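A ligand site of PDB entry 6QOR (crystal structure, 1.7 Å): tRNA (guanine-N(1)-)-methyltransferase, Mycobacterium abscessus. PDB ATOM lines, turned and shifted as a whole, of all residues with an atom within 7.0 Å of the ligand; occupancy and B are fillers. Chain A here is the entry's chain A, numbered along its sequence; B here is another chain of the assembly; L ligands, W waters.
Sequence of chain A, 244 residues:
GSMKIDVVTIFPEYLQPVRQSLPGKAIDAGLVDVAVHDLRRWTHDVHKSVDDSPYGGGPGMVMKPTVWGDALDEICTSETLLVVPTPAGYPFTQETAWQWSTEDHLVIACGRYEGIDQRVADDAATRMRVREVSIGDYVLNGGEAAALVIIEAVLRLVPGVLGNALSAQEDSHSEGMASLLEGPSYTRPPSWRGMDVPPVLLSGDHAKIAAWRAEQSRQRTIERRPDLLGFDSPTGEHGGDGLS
Water W1 lies within hydrogen-bond range of an oxygen (O3) of the ligand and the backbone carbonyl oxygen (O) of Leu 140.
OG of Ser 134 lies within hydrogen-bond range of O1 of the ligand (2.8 Å). N of Leu 140 lies within hydrogen-bond range of O3 of the ligand, 2.8 Å away. The backbone NH (N) of Ile 135 sits at hydrogen-bond distance from an oxygen (O1) of the ligand. The backbone carbonyl oxygen (O) of Tyr 138 sits at hydrogen-bond distance from a nitrogen (N2) of the ligand (3.0 Å). The backbone NH (N) of Gly 136 is in hydrogen-bond range of an oxygen (O1) of the ligand.
The side-chain hydroxyl (OG) of Ser 134 sits at hydrogen-bond distance from the backbone carbonyl oxygen (O) of Gly 136. O of Thr 86 sits close to N of Ser 134 (3.5 Å). O of Ser 134 is in hydrogen-bond range of N of Phe 92 (2.8 Å). The backbone carbonyl oxygen of Ile 135 is in hydrogen-bond range of the side-chain hydroxyl of Tyr 138 (3.2 Å). N of Thr 86 is in hydrogen-bond range of O of Val 133 (3.0 Å). N of Ala 88 sits close to OG1 of Thr 86 (3.3 Å). The backbone NH of Val 133 sits at hydrogen-bond distance from the backbone carbonyl oxygen of Val 84, 3.1 Å away. OE2 of Glu 152 of chain B is in hydrogen-bond range of N of Gly 142, at 3.4 Å.
Merely in contact with the ligand: Ala 146 (3.4 Å), Thr 86 (3.5 Å), Val 139 (3.6 Å), Val 133 (3.6 Å), Pro 87 (3.6 Å), Gly 142 (3.8 Å), Pro 85 (3.9 Å) and Gly 143 (3.9 Å). Hydrophobic or aromatic side chains within 4 Å of the ligand: Pro 85, Pro 87, Ile 135, Leu 140 and Ala 146.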
ATOM      1  N   VAL A  84     -14.264 -23.740   9.453  1.00  0.00           N
ATOM      2  CA  VAL A  84     -13.417 -23.844   8.280  1.00  0.00           C
ATOM      3  C   VAL A  84     -12.248 -22.863   8.439  1.00  0.00           C
ATOM      4  O   VAL A  84     -12.424 -21.666   8.252  1.00  0.00           O
ATOM      5  CB  VAL A  84     -14.187 -23.518   6.974  1.00  0.00           C
ATOM      6  CG1 VAL A  84     -13.294 -23.727   5.757  1.00  0.00           C
ATOM      7  CG2 VAL A  84     -15.458 -24.392   6.876  1.00  0.00           C
ATOM      8  N   PRO A  85     -11.072 -23.360   8.811  1.00  0.00           N
ATOM      9  CA  PRO A  85      -9.975 -22.422   8.924  1.00  0.00           C
ATOM     10  C   PRO A  85      -9.571 -21.919   7.554  1.00  0.00           C
ATOM     11  O   PRO A  85      -9.489 -22.686   6.654  1.00  0.00           O
ATOM     12  CB  PRO A  85      -8.868 -23.259   9.559  1.00  0.00           C
ATOM     13  CG  PRO A  85      -9.566 -24.366  10.235  1.00  0.00           C
ATOM     14  CD  PRO A  85     -10.751 -24.662   9.386  1.00  0.00           C
ATOM     15  N   THR A  86      -9.203 -20.719   7.370  1.00  0.00           N
ATOM     16  CA  THR A  86      -8.927 -19.951   6.169  1.00  0.00           C
ATOM     17  C   THR A  86      -8.418 -18.590   6.590  1.00  0.00           C
ATOM     18  O   THR A  86      -8.838 -18.093   7.551  1.00  0.00           O
ATOM     19  CB  THR A  86     -10.190 -19.783   5.309  1.00  0.00           C
ATOM     20  OG1 THR A  86      -9.867 -19.213   4.058  1.00  0.00           O
ATOM     21  CG2 THR A  86     -11.170 -18.927   5.973  1.00  0.00           C
ATOM     22  N   PRO A  87      -7.299 -18.314   5.707  1.00  0.00           N
ATOM     23  CA  PRO A  87      -6.704 -17.012   5.888  1.00  0.00           C
ATOM     24  C   PRO A  87      -7.704 -15.890   5.614  1.00  0.00           C
ATOM     25  O   PRO A  87      -7.482 -14.786   6.001  1.00  0.00           O
ATOM     26  CB  PRO A  87      -5.567 -16.998   4.869  1.00  0.00           C
ATOM     27  CG  PRO A  87      -5.971 -17.986   3.846  1.00  0.00           C
ATOM     28  CD  PRO A  87      -6.689 -19.047   4.604  1.00  0.00           C
ATOM     29  N   ALA A  88      -8.790 -16.193   4.933  1.00  0.00           N
ATOM     30  CA  ALA A  88      -9.788 -15.188   4.617  1.00  0.00           C
ATOM     31  C   ALA A  88     -10.958 -15.186   5.600  1.00  0.00           C
ATOM     32  O   ALA A  88     -11.988 -14.582   5.316  1.00  0.00           O
ATOM     33  CB  ALA A  88     -10.310 -15.405   3.193  1.00  0.00           C
ATOM     34  N   GLY A  89     -10.793 -15.835   6.749  1.00  0.00           N
ATOM     35  CA  GLY A  89     -11.861 -15.944   7.728  1.00  0.00           C
ATOM     36  C   GLY A  89     -12.015 -14.746   8.646  1.00  0.00           C
ATOM     37  O   GLY A  89     -11.196 -13.828   8.650  1.00  0.00           O
ATOM     38  N   PHE A  92     -10.376 -15.631  14.640  1.00  0.00           N
ATOM     39  CA  PHE A  92     -10.592 -16.507  15.783  1.00  0.00           C
ATOM     40  C   PHE A  92      -9.966 -15.859  17.013  1.00  0.00           C
ATOM     41  O   PHE A  92      -8.754 -15.599  17.038  1.00  0.00           O
ATOM     42  CB  PHE A  92      -9.993 -17.882  15.517  1.00  0.00           C
ATOM     43  CG  PHE A  92     -10.114 -18.839  16.685  1.00  0.00           C
ATOM     44  CD1 PHE A  92     -11.317 -19.487  16.939  1.00  0.00           C
ATOM     45  CD2 PHE A  92      -9.034 -19.067  17.523  1.00  0.00           C
ATOM     46  CE1 PHE A  92     -11.433 -20.365  18.025  1.00  0.00           C
ATOM     47  CE2 PHE A  92      -9.145 -19.936  18.610  1.00  0.00           C
ATOM     48  CZ  PHE A  92     -10.339 -20.597  18.848  1.00  0.00           C
ATOM     49  N   GLY A 111      -8.450 -27.294   4.953  1.00  0.00           N
ATOM     50  CA  GLY A 111      -8.144 -27.160   3.544  1.00  0.00           C
ATOM     51  C   GLY A 111      -6.658 -27.179   3.262  1.00  0.00           C
ATOM     52  O   GLY A 111      -5.822 -27.051   4.166  1.00  0.00           O
ATOM     53  N   VAL A 133     -12.895 -19.021   9.762  1.00  0.00           N
ATOM     54  CA  VAL A 133     -12.086 -18.260  10.705  1.00  0.00           C
ATOM     55  C   VAL A 133     -10.602 -18.340  10.394  1.00  0.00           C
ATOM     56  O   VAL A 133     -10.127 -19.329   9.824  1.00  0.00           O
ATOM     57  CB  VAL A 133     -12.291 -18.726  12.189  1.00  0.00           C
ATOM     58  CG1 VAL A 133     -13.727 -18.460  12.658  1.00  0.00           C
ATOM     59  CG2 VAL A 133     -11.906 -20.196  12.371  1.00  0.00           C
ATOM     60  N   SER A 134      -9.877 -17.296  10.786  1.00  0.00           N
ATOM     61  CA  SER A 134      -8.429 -17.260  10.668  1.00  0.00           C
ATOM     62  C   SER A 134      -7.783 -17.156  12.052  1.00  0.00           C
ATOM     63  O   SER A 134      -8.283 -16.436  12.914  1.00  0.00           O
ATOM     64  CB  SER A 134      -7.977 -16.076   9.808  1.00  0.00           C
ATOM     65  OG  SER A 134      -6.576 -15.943   9.848  1.00  0.00           O
ATOM     66  N   ILE A 135      -6.682 -17.862  12.274  1.00  0.00           N
ATOM     67  CA  ILE A 135      -6.002 -17.779  13.584  1.00  0.00           C
ATOM     68  C   ILE A 135      -4.928 -16.708  13.603  1.00  0.00           C
ATOM     69  O   ILE A 135      -4.388 -16.396  14.657  1.00  0.00           O
ATOM     70  CB  ILE A 135      -5.350 -19.092  14.030  1.00  0.00           C
ATOM     71  CG1 ILE A 135      -4.278 -19.543  13.040  1.00  0.00           C
ATOM     72  CG2 ILE A 135      -6.437 -20.163  14.280  1.00  0.00           C
ATOM     73  CD1 ILE A 135      -3.260 -20.533  13.639  1.00  0.00           C
ATOM     74  N   GLY A 136      -4.619 -16.143  12.436  1.00  0.00           N
ATOM     75  CA  GLY A 136      -3.621 -15.090  12.372  1.00  0.00           C
ATOM     76  C   GLY A 136      -3.292 -14.664  10.962  1.00  0.00           C
ATOM     77  O   GLY A 136      -3.728 -15.290   9.994  1.00  0.00           O
ATOM     78  N   ASP A 137      -2.505 -13.618  10.864  1.00  0.00           N
ATOM     79  CA  ASP A 137      -2.101 -13.046   9.619  1.00  0.00           C
ATOM     80  C   ASP A 137      -0.722 -13.459   9.197  1.00  0.00           C
ATOM     81  O   ASP A 137       0.166 -12.681   9.159  1.00  0.00           O
ATOM     82  CB  ASP A 137      -2.150 -11.532   9.680  1.00  0.00           C
ATOM     83  CG  ASP A 137      -3.528 -11.007   9.670  1.00  0.00           C
ATOM     84  OD1 ASP A 137      -4.391 -11.622   9.049  1.00  0.00           O
ATOM     85  OD2 ASP A 137      -3.720  -9.965  10.262  1.00  0.00           O
ATOM     86  N   TYR A 138      -0.570 -14.720   9.038  1.00  0.00           N
ATOM     87  CA  TYR A 138       0.589 -15.364   8.527  1.00  0.00           C
ATOM     88  C   TYR A 138       0.054 -16.424   7.549  1.00  0.00           C
ATOM     89  O   TYR A 138      -1.074 -16.806   7.589  1.00  0.00           O
ATOM     90  CB  TYR A 138       1.443 -15.987   9.616  1.00  0.00           C
ATOM     91  CG  TYR A 138       0.689 -16.399  10.826  1.00  0.00           C
ATOM     92  CD1 TYR A 138      -0.113 -17.498  10.808  1.00  0.00           C
ATOM     93  CD2 TYR A 138       0.748 -15.670  11.969  1.00  0.00           C
ATOM     94  CE1 TYR A 138      -0.835 -17.873  11.913  1.00  0.00           C
ATOM     95  CE2 TYR A 138       0.030 -16.037  13.076  1.00  0.00           C
ATOM     96  CZ  TYR A 138      -0.752 -17.140  13.037  1.00  0.00           C
ATOM     97  OH  TYR A 138      -1.470 -17.490  14.126  1.00  0.00           O
ATOM     98  N   VAL A 139       0.895 -16.899   6.666  1.00  0.00           N
ATOM     99  CA  VAL A 139       0.435 -17.848   5.691  1.00  0.00           C
ATOM    100  C   VAL A 139       0.909 -19.229   5.967  1.00  0.00           C
ATOM    101  O   VAL A 139       2.036 -19.453   6.131  1.00  0.00           O
ATOM    102  CB  VAL A 139       0.886 -17.464   4.281  1.00  0.00           C
ATOM    103  CG1 VAL A 139       0.362 -18.425   3.262  1.00  0.00           C
ATOM    104  CG2 VAL A 139       0.439 -16.073   3.959  1.00  0.00           C
ATOM    105  N   LEU A 140      -0.035 -20.149   6.039  1.00  0.00           N
ATOM    106  CA  LEU A 140       0.253 -21.562   6.241  1.00  0.00           C
ATOM    107  C   LEU A 140       0.063 -22.315   4.935  1.00  0.00           C
ATOM    108  O   LEU A 140      -0.527 -21.780   3.993  1.00  0.00           O
ATOM    109  CB  LEU A 140      -0.665 -22.140   7.317  1.00  0.00           C
ATOM    110  CG  LEU A 140      -0.682 -21.390   8.649  1.00  0.00           C
ATOM    111  CD1 LEU A 140      -1.784 -21.926   9.552  1.00  0.00           C
ATOM    112  CD2 LEU A 140       0.665 -21.504   9.325  1.00  0.00           C
ATOM    113  N   ASN A 141       0.527 -23.552   4.888  1.00  0.00           N
ATOM    114  CA  ASN A 141       0.311 -24.399   3.718  1.00  0.00           C
ATOM    115  C   ASN A 141      -1.095 -24.972   3.718  1.00  0.00           C
ATOM    116  O   ASN A 141      -1.637 -25.320   2.669  1.00  0.00           O
ATOM    117  CB  ASN A 141       1.330 -25.535   3.675  1.00  0.00           C
ATOM    118  CG  ASN A 141       2.680 -25.088   3.158  1.00  0.00           C
ATOM    119  OD1 ASN A 141       2.781 -24.253   2.251  1.00  0.00           O
ATOM    120  ND2 ASN A 141       3.743 -25.652   3.732  1.00  0.00           N
ATOM    121  N   GLY A 142      -1.680 -25.104   4.900  1.00  0.00           N
ATOM    122  CA  GLY A 142      -3.022 -25.670   5.002  1.00  0.00           C
ATOM    123  C   GLY A 142      -3.582 -25.463   6.384  1.00  0.00           C
ATOM    124  O   GLY A 142      -2.922 -24.903   7.245  1.00  0.00           O
ATOM    125  N   GLY A 143      -4.809 -25.924   6.601  1.00  0.00           N
ATOM    126  CA  GLY A 143      -5.526 -25.654   7.847  1.00  0.00           C
ATOM    127  C   GLY A 143      -5.198 -26.471   9.078  1.00  0.00           C
ATOM    128  O   GLY A 143      -5.724 -26.174  10.164  1.00  0.00           O
ATOM    129  N   GLU A 144      -4.343 -27.487   8.963  1.00  0.00           N
ATOM    130  CA  GLU A 144      -4.116 -28.386  10.101  1.00  0.00           C
ATOM    131  C   GLU A 144      -3.524 -27.697  11.331  1.00  0.00           C
ATOM    132  O   GLU A 144      -3.953 -27.952  12.452  1.00  0.00           O
ATOM    133  CB  GLU A 144      -3.221 -29.546   9.678  1.00  0.00           C
ATOM    134  CG  GLU A 144      -3.911 -30.542   8.761  1.00  0.00           C
ATOM    135  CD  GLU A 144      -3.998 -30.102   7.298  1.00  0.00           C
ATOM    136  OE1 GLU A 144      -3.338 -29.119   6.881  1.00  0.00           O
ATOM    137  OE2 GLU A 144      -4.766 -30.754   6.551  1.00  0.00           O
ATOM    138  N   ALA A 145      -2.539 -26.811  11.137  1.00  0.00           N
ATOM    139  CA  ALA A 145      -1.935 -26.138  12.284  1.00  0.00           C
ATOM    140  C   ALA A 145      -2.968 -25.233  12.955  1.00  0.00           C
ATOM    141  O   ALA A 145      -2.980 -25.092  14.163  1.00  0.00           O
ATOM    142  CB  ALA A 145      -0.688 -25.331  11.881  1.00  0.00           C
ATOM    143  N   ALA A 146      -3.831 -24.633  12.130  1.00  0.00           N
ATOM    144  CA  ALA A 146      -4.904 -23.776  12.634  1.00  0.00           C
ATOM    145  C   ALA A 146      -5.914 -24.617  13.412  1.00  0.00           C
ATOM    146  O   ALA A 146      -6.404 -24.202  14.464  1.00  0.00           O
ATOM    147  CB  ALA A 146      -5.573 -23.023  11.482  1.00  0.00           C
ATOM    148  N   ALA A 147      -6.237 -25.799  12.918  1.00  0.00           N
ATOM    149  CA  ALA A 147      -7.127 -26.713  13.646  1.00  0.00           C
ATOM    150  C   ALA A 147      -6.558 -27.076  15.007  1.00  0.00           C
ATOM    151  O   ALA A 147      -7.273 -27.166  15.998  1.00  0.00           O
ATOM    152  CB  ALA A 147      -7.386 -27.976  12.824  1.00  0.00           C
ATOM    153  N   ILE A 150      -7.045 -24.130  17.332  1.00  0.00           N
ATOM    154  CA  ILE A 150      -8.449 -23.990  17.693  1.00  0.00           C
ATOM    155  C   ILE A 150      -8.881 -25.072  18.688  1.00  0.00           C
ATOM    156  O   ILE A 150      -9.553 -24.804  19.696  1.00  0.00           O
ATOM    157  CB  ILE A 150      -9.337 -24.034  16.426  1.00  0.00           C
ATOM    158  CG1 ILE A 150      -9.145 -22.741  15.630  1.00  0.00           C
ATOM    159  CG2 ILE A 150     -10.802 -24.244  16.779  1.00  0.00           C
ATOM    160  CD1 ILE A 150      -9.613 -22.850  14.178  1.00  0.00           C
ATOM    161  N   GLU B 152       5.852 -23.697  10.354  1.00  0.00           N
ATOM    162  CA  GLU B 152       5.238 -23.868   9.028  1.00  0.00           C
ATOM    163  C   GLU B 152       5.284 -22.577   8.219  1.00  0.00           C
ATOM    164  O   GLU B 152       5.617 -22.579   7.035  1.00  0.00           O
ATOM    165  CB  GLU B 152       3.793 -24.372   9.144  1.00  0.00           C
ATOM    166  CG  GLU B 152       3.134 -24.535   7.788  1.00  0.00           C
ATOM    167  CD  GLU B 152       1.803 -25.264   7.866  1.00  0.00           C
ATOM    168  OE1 GLU B 152       1.563 -25.961   8.875  1.00  0.00           O
ATOM    169  OE2 GLU B 152       1.005 -25.146   6.930  1.00  0.00           O
ATOM    170  N   ARG B 156       8.066 -22.358   4.688  1.00  0.00           N
ATOM    171  CA  ARG B 156       7.564 -22.310   3.322  1.00  0.00           C
ATOM    172  C   ARG B 156       8.131 -21.108   2.557  1.00  0.00           C
ATOM    173  O   ARG B 156       7.995 -21.028   1.339  1.00  0.00           O
ATOM    174  CB  ARG B 156       6.032 -22.311   3.311  1.00  0.00           C
ATOM    175  CG  ARG B 156       5.390 -21.182   4.069  1.00  0.00           C
ATOM    176  CD  ARG B 156       3.873 -21.358   4.112  1.00  0.00           C
ATOM    177  NE  ARG B 156       3.272 -21.351   2.786  1.00  0.00           N
ATOM    178  CZ  ARG B 156       3.128 -20.262   2.022  1.00  0.00           C
ATOM    179  NH1 ARG B 156       3.576 -19.078   2.439  1.00  0.00           N
ATOM    180  NH2 ARG B 156       2.554 -20.366   0.833  1.00  0.00           N
HETATM  181  C1  LIG L   1      -4.239 -19.536   7.536  1.00  0.00           C
HETATM  182  O1  LIG L   1      -5.281 -18.397   9.861  1.00  0.00           O
HETATM  183  N1  LIG L   1      -5.764 -19.585   9.440  1.00  0.00           N
HETATM  184  O2  LIG L   1      -6.641 -20.144  10.086  1.00  0.00           O
HETATM  185  C2  LIG L   1      -5.250 -20.160   8.250  1.00  0.00           C
HETATM  186  C3  LIG L   1      -5.763 -21.376   7.820  1.00  0.00           C
HETATM  187  C4  LIG L   1      -5.254 -21.961   6.671  1.00  0.00           C
HETATM  188  C5  LIG L   1      -4.252 -21.341   5.948  1.00  0.00           C
HETATM  189  C6  LIG L   1      -3.751 -20.132   6.383  1.00  0.00           C
HETATM  190  O3  LIG L   1      -2.750 -19.469   5.677  1.00  0.00           O
HETATM  191  N2  LIG L   1      -3.683 -18.298   7.932  1.00  0.00           N
HETATM  192  O   HOH W   1      -2.746 -20.040   3.125  1.00  0.00           O
